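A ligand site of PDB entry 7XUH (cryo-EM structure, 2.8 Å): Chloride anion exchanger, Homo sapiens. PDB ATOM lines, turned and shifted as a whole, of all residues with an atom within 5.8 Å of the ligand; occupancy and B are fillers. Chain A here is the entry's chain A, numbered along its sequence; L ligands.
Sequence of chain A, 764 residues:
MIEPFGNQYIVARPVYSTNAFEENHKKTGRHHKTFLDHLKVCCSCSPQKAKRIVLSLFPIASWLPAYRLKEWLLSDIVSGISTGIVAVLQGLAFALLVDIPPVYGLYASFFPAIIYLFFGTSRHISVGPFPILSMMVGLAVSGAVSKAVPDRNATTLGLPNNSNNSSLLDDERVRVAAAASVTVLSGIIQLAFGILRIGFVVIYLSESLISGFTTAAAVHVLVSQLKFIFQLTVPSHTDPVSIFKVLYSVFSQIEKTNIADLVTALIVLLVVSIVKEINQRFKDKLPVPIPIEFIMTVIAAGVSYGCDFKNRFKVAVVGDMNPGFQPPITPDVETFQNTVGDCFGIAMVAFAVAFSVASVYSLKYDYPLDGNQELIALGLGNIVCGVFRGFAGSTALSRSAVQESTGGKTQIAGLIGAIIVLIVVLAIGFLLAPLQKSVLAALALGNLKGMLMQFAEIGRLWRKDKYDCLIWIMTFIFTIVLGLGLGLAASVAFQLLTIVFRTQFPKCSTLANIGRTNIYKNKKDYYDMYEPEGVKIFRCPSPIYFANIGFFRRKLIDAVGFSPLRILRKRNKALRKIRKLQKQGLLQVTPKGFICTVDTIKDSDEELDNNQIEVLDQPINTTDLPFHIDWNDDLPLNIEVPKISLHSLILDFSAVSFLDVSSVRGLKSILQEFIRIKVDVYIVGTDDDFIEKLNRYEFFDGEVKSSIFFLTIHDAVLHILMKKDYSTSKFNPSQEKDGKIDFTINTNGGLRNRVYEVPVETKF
O1 of the ligand sits close to SD of Met 451 (3.6 Å). Merely in contact with the ligand: Phe 213 (3.1 Å), Ser 356 (3.2 Å), Leu 205 (3.3 Å), Pro 131 (3.5 Å), Ala 352 (3.6 Å), Val 353 (3.6 Å), Phe 130 (3.6 Å), Asn 447 (3.6 Å), Ile 132 (3.7 Å), Ile 210 (3.7 Å), Ala 396 (3.7 Å) and Leu 397 (3.9 Å). Hydrophobic or aromatic side chains that line the ligand: Phe 130, Pro 131, Ile 132, Leu 205, Ile 210, Phe 213, Ala 352, Val 353, Ala 396, Leu 397 and Met 451. The nearest printed residue that does not touch the ligand is Leu 488 (4.1 Å).
An oxygen (O4) of the ligand is in hydrogen-bond range of the backbone NH (N) of Ser 398, at 3.2 Å. OG of Ser 398 sits at hydrogen-bond distance from O4 of the ligand (2.7 Å). The side-chain hydroxyl (OG1) of Thr 214 lies within hydrogen-bond range of an oxygen (O2) of the ligand, 3.4 Å away.
O of Ala 352 lies within hydrogen-bond range of OG of Ser 356 (3.4 Å). The side-chain hydroxyl (OG) of Ser 356 lies within hydrogen-bond range of the backbone carbonyl oxygen (O) of Val 353, at 2.9 Å. The side-chain hydroxyl of Thr 214 sits at hydrogen-bond distance from the backbone carbonyl oxygen of Ile 210 (2.8 Å).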
ATOM      1  N   GLN A  90      39.765  -2.668   6.479  1.00  0.00           N
ATOM      2  CA  GLN A  90      39.069  -3.946   6.569  1.00  0.00           C
ATOM      3  C   GLN A  90      39.928  -5.101   6.079  1.00  0.00           C
ATOM      4  O   GLN A  90      39.796  -6.217   6.584  1.00  0.00           O
ATOM      5  CB  GLN A  90      37.767  -3.888   5.792  1.00  0.00           C
ATOM      6  CG  GLN A  90      36.694  -3.064   6.462  1.00  0.00           C
ATOM      7  CD  GLN A  90      35.334  -3.329   5.881  1.00  0.00           C
ATOM      8  OE1 GLN A  90      35.199  -4.081   4.917  1.00  0.00           O
ATOM      9  NE2 GLN A  90      34.318  -2.709   6.441  1.00  0.00           N
ATOM     10  N   PHE A  94      40.541  -8.264   8.534  1.00  0.00           N
ATOM     11  CA  PHE A  94      40.005  -9.588   8.266  1.00  0.00           C
ATOM     12  C   PHE A  94      41.087 -10.638   8.060  1.00  0.00           C
ATOM     13  O   PHE A  94      40.760 -11.829   8.025  1.00  0.00           O
ATOM     14  CB  PHE A  94      39.078  -9.589   7.040  1.00  0.00           C
ATOM     15  CG  PHE A  94      37.908  -8.653   7.147  1.00  0.00           C
ATOM     16  CD1 PHE A  94      37.382  -8.292   8.383  1.00  0.00           C
ATOM     17  CD2 PHE A  94      37.326  -8.145   6.003  1.00  0.00           C
ATOM     18  CE1 PHE A  94      36.325  -7.426   8.458  1.00  0.00           C
ATOM     19  CE2 PHE A  94      36.265  -7.287   6.084  1.00  0.00           C
ATOM     20  CZ  PHE A  94      35.763  -6.931   7.314  1.00  0.00           C
ATOM     21  N   PHE A 130      35.212 -10.194   3.334  1.00  0.00           N
ATOM     22  CA  PHE A 130      34.178  -9.873   4.310  1.00  0.00           C
ATOM     23  C   PHE A 130      34.223 -10.927   5.417  1.00  0.00           C
ATOM     24  O   PHE A 130      34.706 -12.036   5.150  1.00  0.00           O
ATOM     25  CB  PHE A 130      32.792  -9.749   3.623  1.00  0.00           C
ATOM     26  CG  PHE A 130      32.195 -11.031   3.130  1.00  0.00           C
ATOM     27  CD1 PHE A 130      32.481 -11.494   1.866  1.00  0.00           C
ATOM     28  CD2 PHE A 130      31.261 -11.709   3.892  1.00  0.00           C
ATOM     29  CE1 PHE A 130      31.898 -12.642   1.394  1.00  0.00           C
ATOM     30  CE2 PHE A 130      30.678 -12.858   3.420  1.00  0.00           C
ATOM     31  CZ  PHE A 130      30.989 -13.323   2.176  1.00  0.00           C
ATOM     32  N   PRO A 131      33.771 -10.616   6.652  1.00  0.00           N
ATOM     33  CA  PRO A 131      34.188 -11.427   7.829  1.00  0.00           C
ATOM     34  C   PRO A 131      33.756 -12.889   7.848  1.00  0.00           C
ATOM     35  O   PRO A 131      34.526 -13.731   8.328  1.00  0.00           O
ATOM     36  CB  PRO A 131      33.551 -10.675   8.999  1.00  0.00           C
ATOM     37  CG  PRO A 131      33.344  -9.350   8.549  1.00  0.00           C
ATOM     38  CD  PRO A 131      33.092  -9.383   7.102  1.00  0.00           C
ATOM     39  N   ILE A 132      32.547 -13.194   7.386  1.00  0.00           N
ATOM     40  CA  ILE A 132      32.052 -14.575   7.459  1.00  0.00           C
ATOM     41  C   ILE A 132      32.860 -15.477   6.542  1.00  0.00           C
ATOM     42  O   ILE A 132      33.222 -16.607   6.917  1.00  0.00           O
ATOM     43  CB  ILE A 132      30.556 -14.595   7.125  1.00  0.00           C
ATOM     44  CG1 ILE A 132      29.767 -13.909   8.224  1.00  0.00           C
ATOM     45  CG2 ILE A 132      30.042 -16.008   6.948  1.00  0.00           C
ATOM     46  CD1 ILE A 132      28.339 -13.698   7.865  1.00  0.00           C
ATOM     47  N   LEU A 205      17.169 -20.417  -1.719  1.00  0.00           N
ATOM     48  CA  LEU A 205      17.430 -19.852  -0.400  1.00  0.00           C
ATOM     49  C   LEU A 205      16.297 -18.888  -0.089  1.00  0.00           C
ATOM     50  O   LEU A 205      16.227 -17.799  -0.678  1.00  0.00           O
ATOM     51  CB  LEU A 205      18.780 -19.143  -0.371  1.00  0.00           C
ATOM     52  CG  LEU A 205      20.014 -19.880   0.151  1.00  0.00           C
ATOM     53  CD1 LEU A 205      20.312 -21.137  -0.633  1.00  0.00           C
ATOM     54  CD2 LEU A 205      21.197 -18.959   0.071  1.00  0.00           C
ATOM     55  N   LEU A 209      15.548 -18.642   5.869  1.00  0.00           N
ATOM     56  CA  LEU A 209      16.848 -19.297   5.952  1.00  0.00           C
ATOM     57  C   LEU A 209      17.970 -18.270   5.998  1.00  0.00           C
ATOM     58  O   LEU A 209      18.921 -18.419   6.777  1.00  0.00           O
ATOM     59  CB  LEU A 209      17.036 -20.238   4.773  1.00  0.00           C
ATOM     60  CG  LEU A 209      18.253 -21.154   4.735  1.00  0.00           C
ATOM     61  CD1 LEU A 209      17.839 -22.526   4.302  1.00  0.00           C
ATOM     62  CD2 LEU A 209      19.298 -20.620   3.781  1.00  0.00           C
ATOM     63  N   ILE A 210      17.866 -17.228   5.183  1.00  0.00           N
ATOM     64  CA  ILE A 210      18.902 -16.199   5.136  1.00  0.00           C
ATOM     65  C   ILE A 210      18.934 -15.421   6.443  1.00  0.00           C
ATOM     66  O   ILE A 210      20.010 -15.121   6.970  1.00  0.00           O
ATOM     67  CB  ILE A 210      18.674 -15.296   3.909  1.00  0.00           C
ATOM     68  CG1 ILE A 210      18.985 -16.068   2.632  1.00  0.00           C
ATOM     69  CG2 ILE A 210      19.557 -14.071   3.953  1.00  0.00           C
ATOM     70  CD1 ILE A 210      18.464 -15.397   1.399  1.00  0.00           C
ATOM     71  N   PHE A 213      20.467 -17.847   9.210  1.00  0.00           N
ATOM     72  CA  PHE A 213      21.898 -18.003   8.962  1.00  0.00           C
ATOM     73  C   PHE A 213      22.668 -16.740   9.299  1.00  0.00           C
ATOM     74  O   PHE A 213      23.737 -16.807   9.895  1.00  0.00           O
ATOM     75  CB  PHE A 213      22.124 -18.392   7.498  1.00  0.00           C
ATOM     76  CG  PHE A 213      23.560 -18.628   7.146  1.00  0.00           C
ATOM     77  CD1 PHE A 213      24.164 -19.829   7.432  1.00  0.00           C
ATOM     78  CD2 PHE A 213      24.297 -17.649   6.500  1.00  0.00           C
ATOM     79  CE1 PHE A 213      25.480 -20.052   7.105  1.00  0.00           C
ATOM     80  CE2 PHE A 213      25.617 -17.858   6.176  1.00  0.00           C
ATOM     81  CZ  PHE A 213      26.202 -19.065   6.475  1.00  0.00           C
ATOM     82  N   THR A 214      22.120 -15.583   8.927  1.00  0.00           N
ATOM     83  CA  THR A 214      22.790 -14.315   9.182  1.00  0.00           C
ATOM     84  C   THR A 214      22.853 -14.010  10.677  1.00  0.00           C
ATOM     85  O   THR A 214      23.889 -13.561  11.179  1.00  0.00           O
ATOM     86  CB  THR A 214      22.046 -13.228   8.410  1.00  0.00           C
ATOM     87  OG1 THR A 214      22.266 -13.425   7.008  1.00  0.00           O
ATOM     88  CG2 THR A 214      22.484 -11.859   8.783  1.00  0.00           C
ATOM     89  N   MET A 348      29.726 -21.089  -2.814  1.00  0.00           N
ATOM     90  CA  MET A 348      28.289 -20.817  -2.833  1.00  0.00           C
ATOM     91  C   MET A 348      27.917 -19.631  -1.962  1.00  0.00           C
ATOM     92  O   MET A 348      27.099 -18.796  -2.363  1.00  0.00           O
ATOM     93  CB  MET A 348      27.510 -22.063  -2.414  1.00  0.00           C
ATOM     94  CG  MET A 348      27.553 -23.184  -3.451  1.00  0.00           C
ATOM     95  SD  MET A 348      26.765 -22.763  -5.009  1.00  0.00           S
ATOM     96  CE  MET A 348      28.171 -22.693  -6.116  1.00  0.00           C
ATOM     97  N   VAL A 349      28.524 -19.521  -0.779  1.00  0.00           N
ATOM     98  CA  VAL A 349      28.220 -18.402   0.119  1.00  0.00           C
ATOM     99  C   VAL A 349      28.707 -17.091  -0.473  1.00  0.00           C
ATOM    100  O   VAL A 349      28.002 -16.069  -0.426  1.00  0.00           O
ATOM    101  CB  VAL A 349      28.811 -18.674   1.513  1.00  0.00           C
ATOM    102  CG1 VAL A 349      28.898 -17.419   2.352  1.00  0.00           C
ATOM    103  CG2 VAL A 349      27.969 -19.697   2.235  1.00  0.00           C
ATOM    104  N   ALA A 352      26.317 -16.109  -3.386  1.00  0.00           N
ATOM    105  CA  ALA A 352      24.992 -15.725  -2.908  1.00  0.00           C
ATOM    106  C   ALA A 352      24.998 -14.348  -2.260  1.00  0.00           C
ATOM    107  O   ALA A 352      24.103 -13.526  -2.518  1.00  0.00           O
ATOM    108  CB  ALA A 352      24.461 -16.777  -1.948  1.00  0.00           C
ATOM    109  N   VAL A 353      26.019 -14.071  -1.434  1.00  0.00           N
ATOM    110  CA  VAL A 353      26.127 -12.765  -0.792  1.00  0.00           C
ATOM    111  C   VAL A 353      26.345 -11.666  -1.833  1.00  0.00           C
ATOM    112  O   VAL A 353      25.670 -10.623  -1.787  1.00  0.00           O
ATOM    113  CB  VAL A 353      27.262 -12.781   0.254  1.00  0.00           C
ATOM    114  CG1 VAL A 353      27.600 -11.387   0.725  1.00  0.00           C
ATOM    115  CG2 VAL A 353      26.861 -13.617   1.431  1.00  0.00           C
ATOM    116  N   SER A 356      23.068 -11.043  -3.890  1.00  0.00           N
ATOM    117  CA  SER A 356      22.021 -10.368  -3.132  1.00  0.00           C
ATOM    118  C   SER A 356      22.361  -8.910  -2.858  1.00  0.00           C
ATOM    119  O   SER A 356      21.458  -8.073  -2.817  1.00  0.00           O
ATOM    120  CB  SER A 356      21.784 -11.073  -1.805  1.00  0.00           C
ATOM    121  OG  SER A 356      22.870 -10.828  -0.944  1.00  0.00           O
ATOM    122  N   VAL A 357      23.640  -8.592  -2.659  1.00  0.00           N
ATOM    123  CA  VAL A 357      23.984  -7.186  -2.433  1.00  0.00           C
ATOM    124  C   VAL A 357      23.922  -6.396  -3.741  1.00  0.00           C
ATOM    125  O   VAL A 357      23.488  -5.242  -3.767  1.00  0.00           O
ATOM    126  CB  VAL A 357      25.354  -7.084  -1.740  1.00  0.00           C
ATOM    127  CG1 VAL A 357      25.775  -5.650  -1.541  1.00  0.00           C
ATOM    128  CG2 VAL A 357      25.287  -7.729  -0.389  1.00  0.00           C
ATOM    129  N   ALA A 396      31.439  -6.893   0.380  1.00  0.00           N
ATOM    130  CA  ALA A 396      30.972  -6.703   1.740  1.00  0.00           C
ATOM    131  C   ALA A 396      29.867  -5.666   1.719  1.00  0.00           C
ATOM    132  O   ALA A 396      29.890  -4.742   0.914  1.00  0.00           O
ATOM    133  CB  ALA A 396      32.100  -6.234   2.657  1.00  0.00           C
ATOM    134  N   LEU A 397      28.895  -5.824   2.619  1.00  0.00           N
ATOM    135  CA  LEU A 397      27.715  -4.957   2.585  1.00  0.00           C
ATOM    136  C   LEU A 397      28.046  -3.558   3.076  1.00  0.00           C
ATOM    137  O   LEU A 397      27.564  -2.571   2.515  1.00  0.00           O
ATOM    138  CB  LEU A 397      26.595  -5.584   3.423  1.00  0.00           C
ATOM    139  CG  LEU A 397      25.172  -5.072   3.245  1.00  0.00           C
ATOM    140  CD1 LEU A 397      24.225  -6.250   3.284  1.00  0.00           C
ATOM    141  CD2 LEU A 397      24.797  -4.087   4.336  1.00  0.00           C
ATOM    142  N   SER A 398      28.902  -3.450   4.098  1.00  0.00           N
ATOM    143  CA  SER A 398      29.231  -2.143   4.652  1.00  0.00           C
ATOM    144  C   SER A 398      30.130  -1.338   3.727  1.00  0.00           C
ATOM    145  O   SER A 398      29.941  -0.136   3.564  1.00  0.00           O
ATOM    146  CB  SER A 398      29.892  -2.317   6.014  1.00  0.00           C
ATOM    147  OG  SER A 398      30.814  -3.385   5.983  1.00  0.00           O
ATOM    148  N   ARG A 399      31.085  -2.008   3.082  1.00  0.00           N
ATOM    149  CA  ARG A 399      31.980  -1.313   2.156  1.00  0.00           C
ATOM    150  C   ARG A 399      31.248  -0.892   0.894  1.00  0.00           C
ATOM    151  O   ARG A 399      31.499   0.185   0.346  1.00  0.00           O
ATOM    152  CB  ARG A 399      33.166  -2.207   1.834  1.00  0.00           C
ATOM    153  CG  ARG A 399      34.434  -1.485   1.448  1.00  0.00           C
ATOM    154  CD  ARG A 399      35.558  -2.471   1.194  1.00  0.00           C
ATOM    155  NE  ARG A 399      35.076  -3.643   0.494  1.00  0.00           N
ATOM    156  CZ  ARG A 399      35.221  -4.890   0.937  1.00  0.00           C
ATOM    157  NH1 ARG A 399      35.838  -5.119   2.089  1.00  0.00           N
ATOM    158  NH2 ARG A 399      34.734  -5.900   0.244  1.00  0.00           N
ATOM    159  N   ASN A 447      29.692  -3.265  12.636  1.00  0.00           N
ATOM    160  CA  ASN A 447      28.767  -3.629  11.568  1.00  0.00           C
ATOM    161  C   ASN A 447      27.905  -4.821  11.930  1.00  0.00           C
ATOM    162  O   ASN A 447      27.378  -5.484  11.023  1.00  0.00           O
ATOM    163  CB  ASN A 447      29.545  -3.909  10.286  1.00  0.00           C
ATOM    164  CG  ASN A 447      30.503  -2.783   9.939  1.00  0.00           C
ATOM    165  OD1 ASN A 447      30.128  -1.620   9.940  1.00  0.00           O
ATOM    166  ND2 ASN A 447      31.742  -3.137   9.633  1.00  0.00           N
ATOM    167  N   LEU A 448      27.739  -5.114  13.211  1.00  0.00           N
ATOM    168  CA  LEU A 448      26.933  -6.239  13.656  1.00  0.00           C
ATOM    169  C   LEU A 448      25.535  -5.844  14.103  1.00  0.00           C
ATOM    170  O   LEU A 448      24.777  -6.713  14.538  1.00  0.00           O
ATOM    171  CB  LEU A 448      27.617  -6.956  14.819  1.00  0.00           C
ATOM    172  CG  LEU A 448      28.952  -7.677  14.635  1.00  0.00           C
ATOM    173  CD1 LEU A 448      29.104  -8.705  15.721  1.00  0.00           C
ATOM    174  CD2 LEU A 448      29.072  -8.315  13.272  1.00  0.00           C
ATOM    175  N   MET A 451      22.672  -7.150  11.733  1.00  0.00           N
ATOM    176  CA  MET A 451      22.549  -8.599  11.758  1.00  0.00           C
ATOM    177  C   MET A 451      21.979  -9.095  13.072  1.00  0.00           C
ATOM    178  O   MET A 451      21.238 -10.078  13.081  1.00  0.00           O
ATOM    179  CB  MET A 451      23.910  -9.239  11.497  1.00  0.00           C
ATOM    180  CG  MET A 451      24.467  -8.996  10.116  1.00  0.00           C
ATOM    181  SD  MET A 451      25.627 -10.272   9.598  1.00  0.00           S
ATOM    182  CE  MET A 451      27.023  -9.886  10.621  1.00  0.00           C
ATOM    183  N   LEU A 488      24.579 -24.758   6.776  1.00  0.00           N
ATOM    184  CA  LEU A 488      23.825 -24.275   5.616  1.00  0.00           C
ATOM    185  C   LEU A 488      23.310 -25.444   4.778  1.00  0.00           C
ATOM    186  O   LEU A 488      22.168 -25.409   4.303  1.00  0.00           O
ATOM    187  CB  LEU A 488      24.701 -23.360   4.779  1.00  0.00           C
ATOM    188  CG  LEU A 488      24.006 -22.589   3.662  1.00  0.00           C
ATOM    189  CD1 LEU A 488      23.133 -21.504   4.235  1.00  0.00           C
ATOM    190  CD2 LEU A 488      25.029 -22.000   2.725  1.00  0.00           C
HETATM  191  C1  LIG L   1      25.875  -9.236   6.179  1.00  0.00           C
HETATM  192  C2  LIG L   1      28.290  -8.263   7.456  1.00  0.00           C
HETATM  193  C3  LIG L   1      26.902 -11.288   5.504  1.00  0.00           C
HETATM  194  C4  LIG L   1      26.762  -7.374   7.238  1.00  0.00           C
HETATM  195  C5  LIG L   1      23.282  -9.333   5.470  1.00  0.00           C
HETATM  196  C6  LIG L   1      23.789 -11.896   2.976  1.00  0.00           C
HETATM  197  C7  LIG L   1      23.235 -13.166   2.308  1.00  0.00           C
HETATM  198  C8  LIG L   1      23.121 -15.543   2.098  1.00  0.00           C
HETATM  199  C9  LIG L   1      30.008  -6.547   6.815  1.00  0.00           C
HETATM  200  C10 LIG L   1      21.848 -14.133   0.605  1.00  0.00           C
HETATM  201  C11 LIG L   1      27.110  -9.987   6.151  1.00  0.00           C
HETATM  202  C12 LIG L   1      28.346  -9.529   6.672  1.00  0.00           C
HETATM  203  C13 LIG L   1      24.661 -10.022   5.501  1.00  0.00           C
HETATM  204  C14 LIG L   1      24.928 -11.202   5.041  1.00  0.00           C
HETATM  205  C15 LIG L   1      25.885 -11.790   5.022  1.00  0.00           C
HETATM  206  C16 LIG L   1      29.579  -7.545   7.900  1.00  0.00           C
HETATM  207  C17 LIG L   1      29.550 -10.417   6.793  1.00  0.00           C
HETATM  208  C18 LIG L   1      23.618 -14.444   2.731  1.00  0.00           C
HETATM  209  C19 LIG L   1      22.353 -13.031   1.250  1.00  0.00           C
HETATM  210  C20 LIG L   1      22.239 -15.413   1.032  1.00  0.00           C
HETATM  211  C21 LIG L   1      23.559 -16.939   2.562  1.00  0.00           C
HETATM  212  F1  LIG L   1      22.546 -17.541   3.224  1.00  0.00           F
HETATM  213  F2  LIG L   1      23.922 -17.685   1.480  1.00  0.00           F
HETATM  214  F3  LIG L   1      24.631 -16.780   3.389  1.00  0.00           F
HETATM  215  O1  LIG L   1      25.735  -8.163   6.628  1.00  0.00           O
HETATM  216  O2  LIG L   1      23.821 -11.918   4.438  1.00  0.00           O
HETATM  217  O3  LIG L   1      26.611  -6.244   7.546  1.00  0.00           O
HETATM  218  O4  LIG L   1      29.270  -5.563   6.535  1.00  0.00           O
HETATM  219  O5  LIG L   1      31.102  -6.705   6.208  1.00  0.00           O
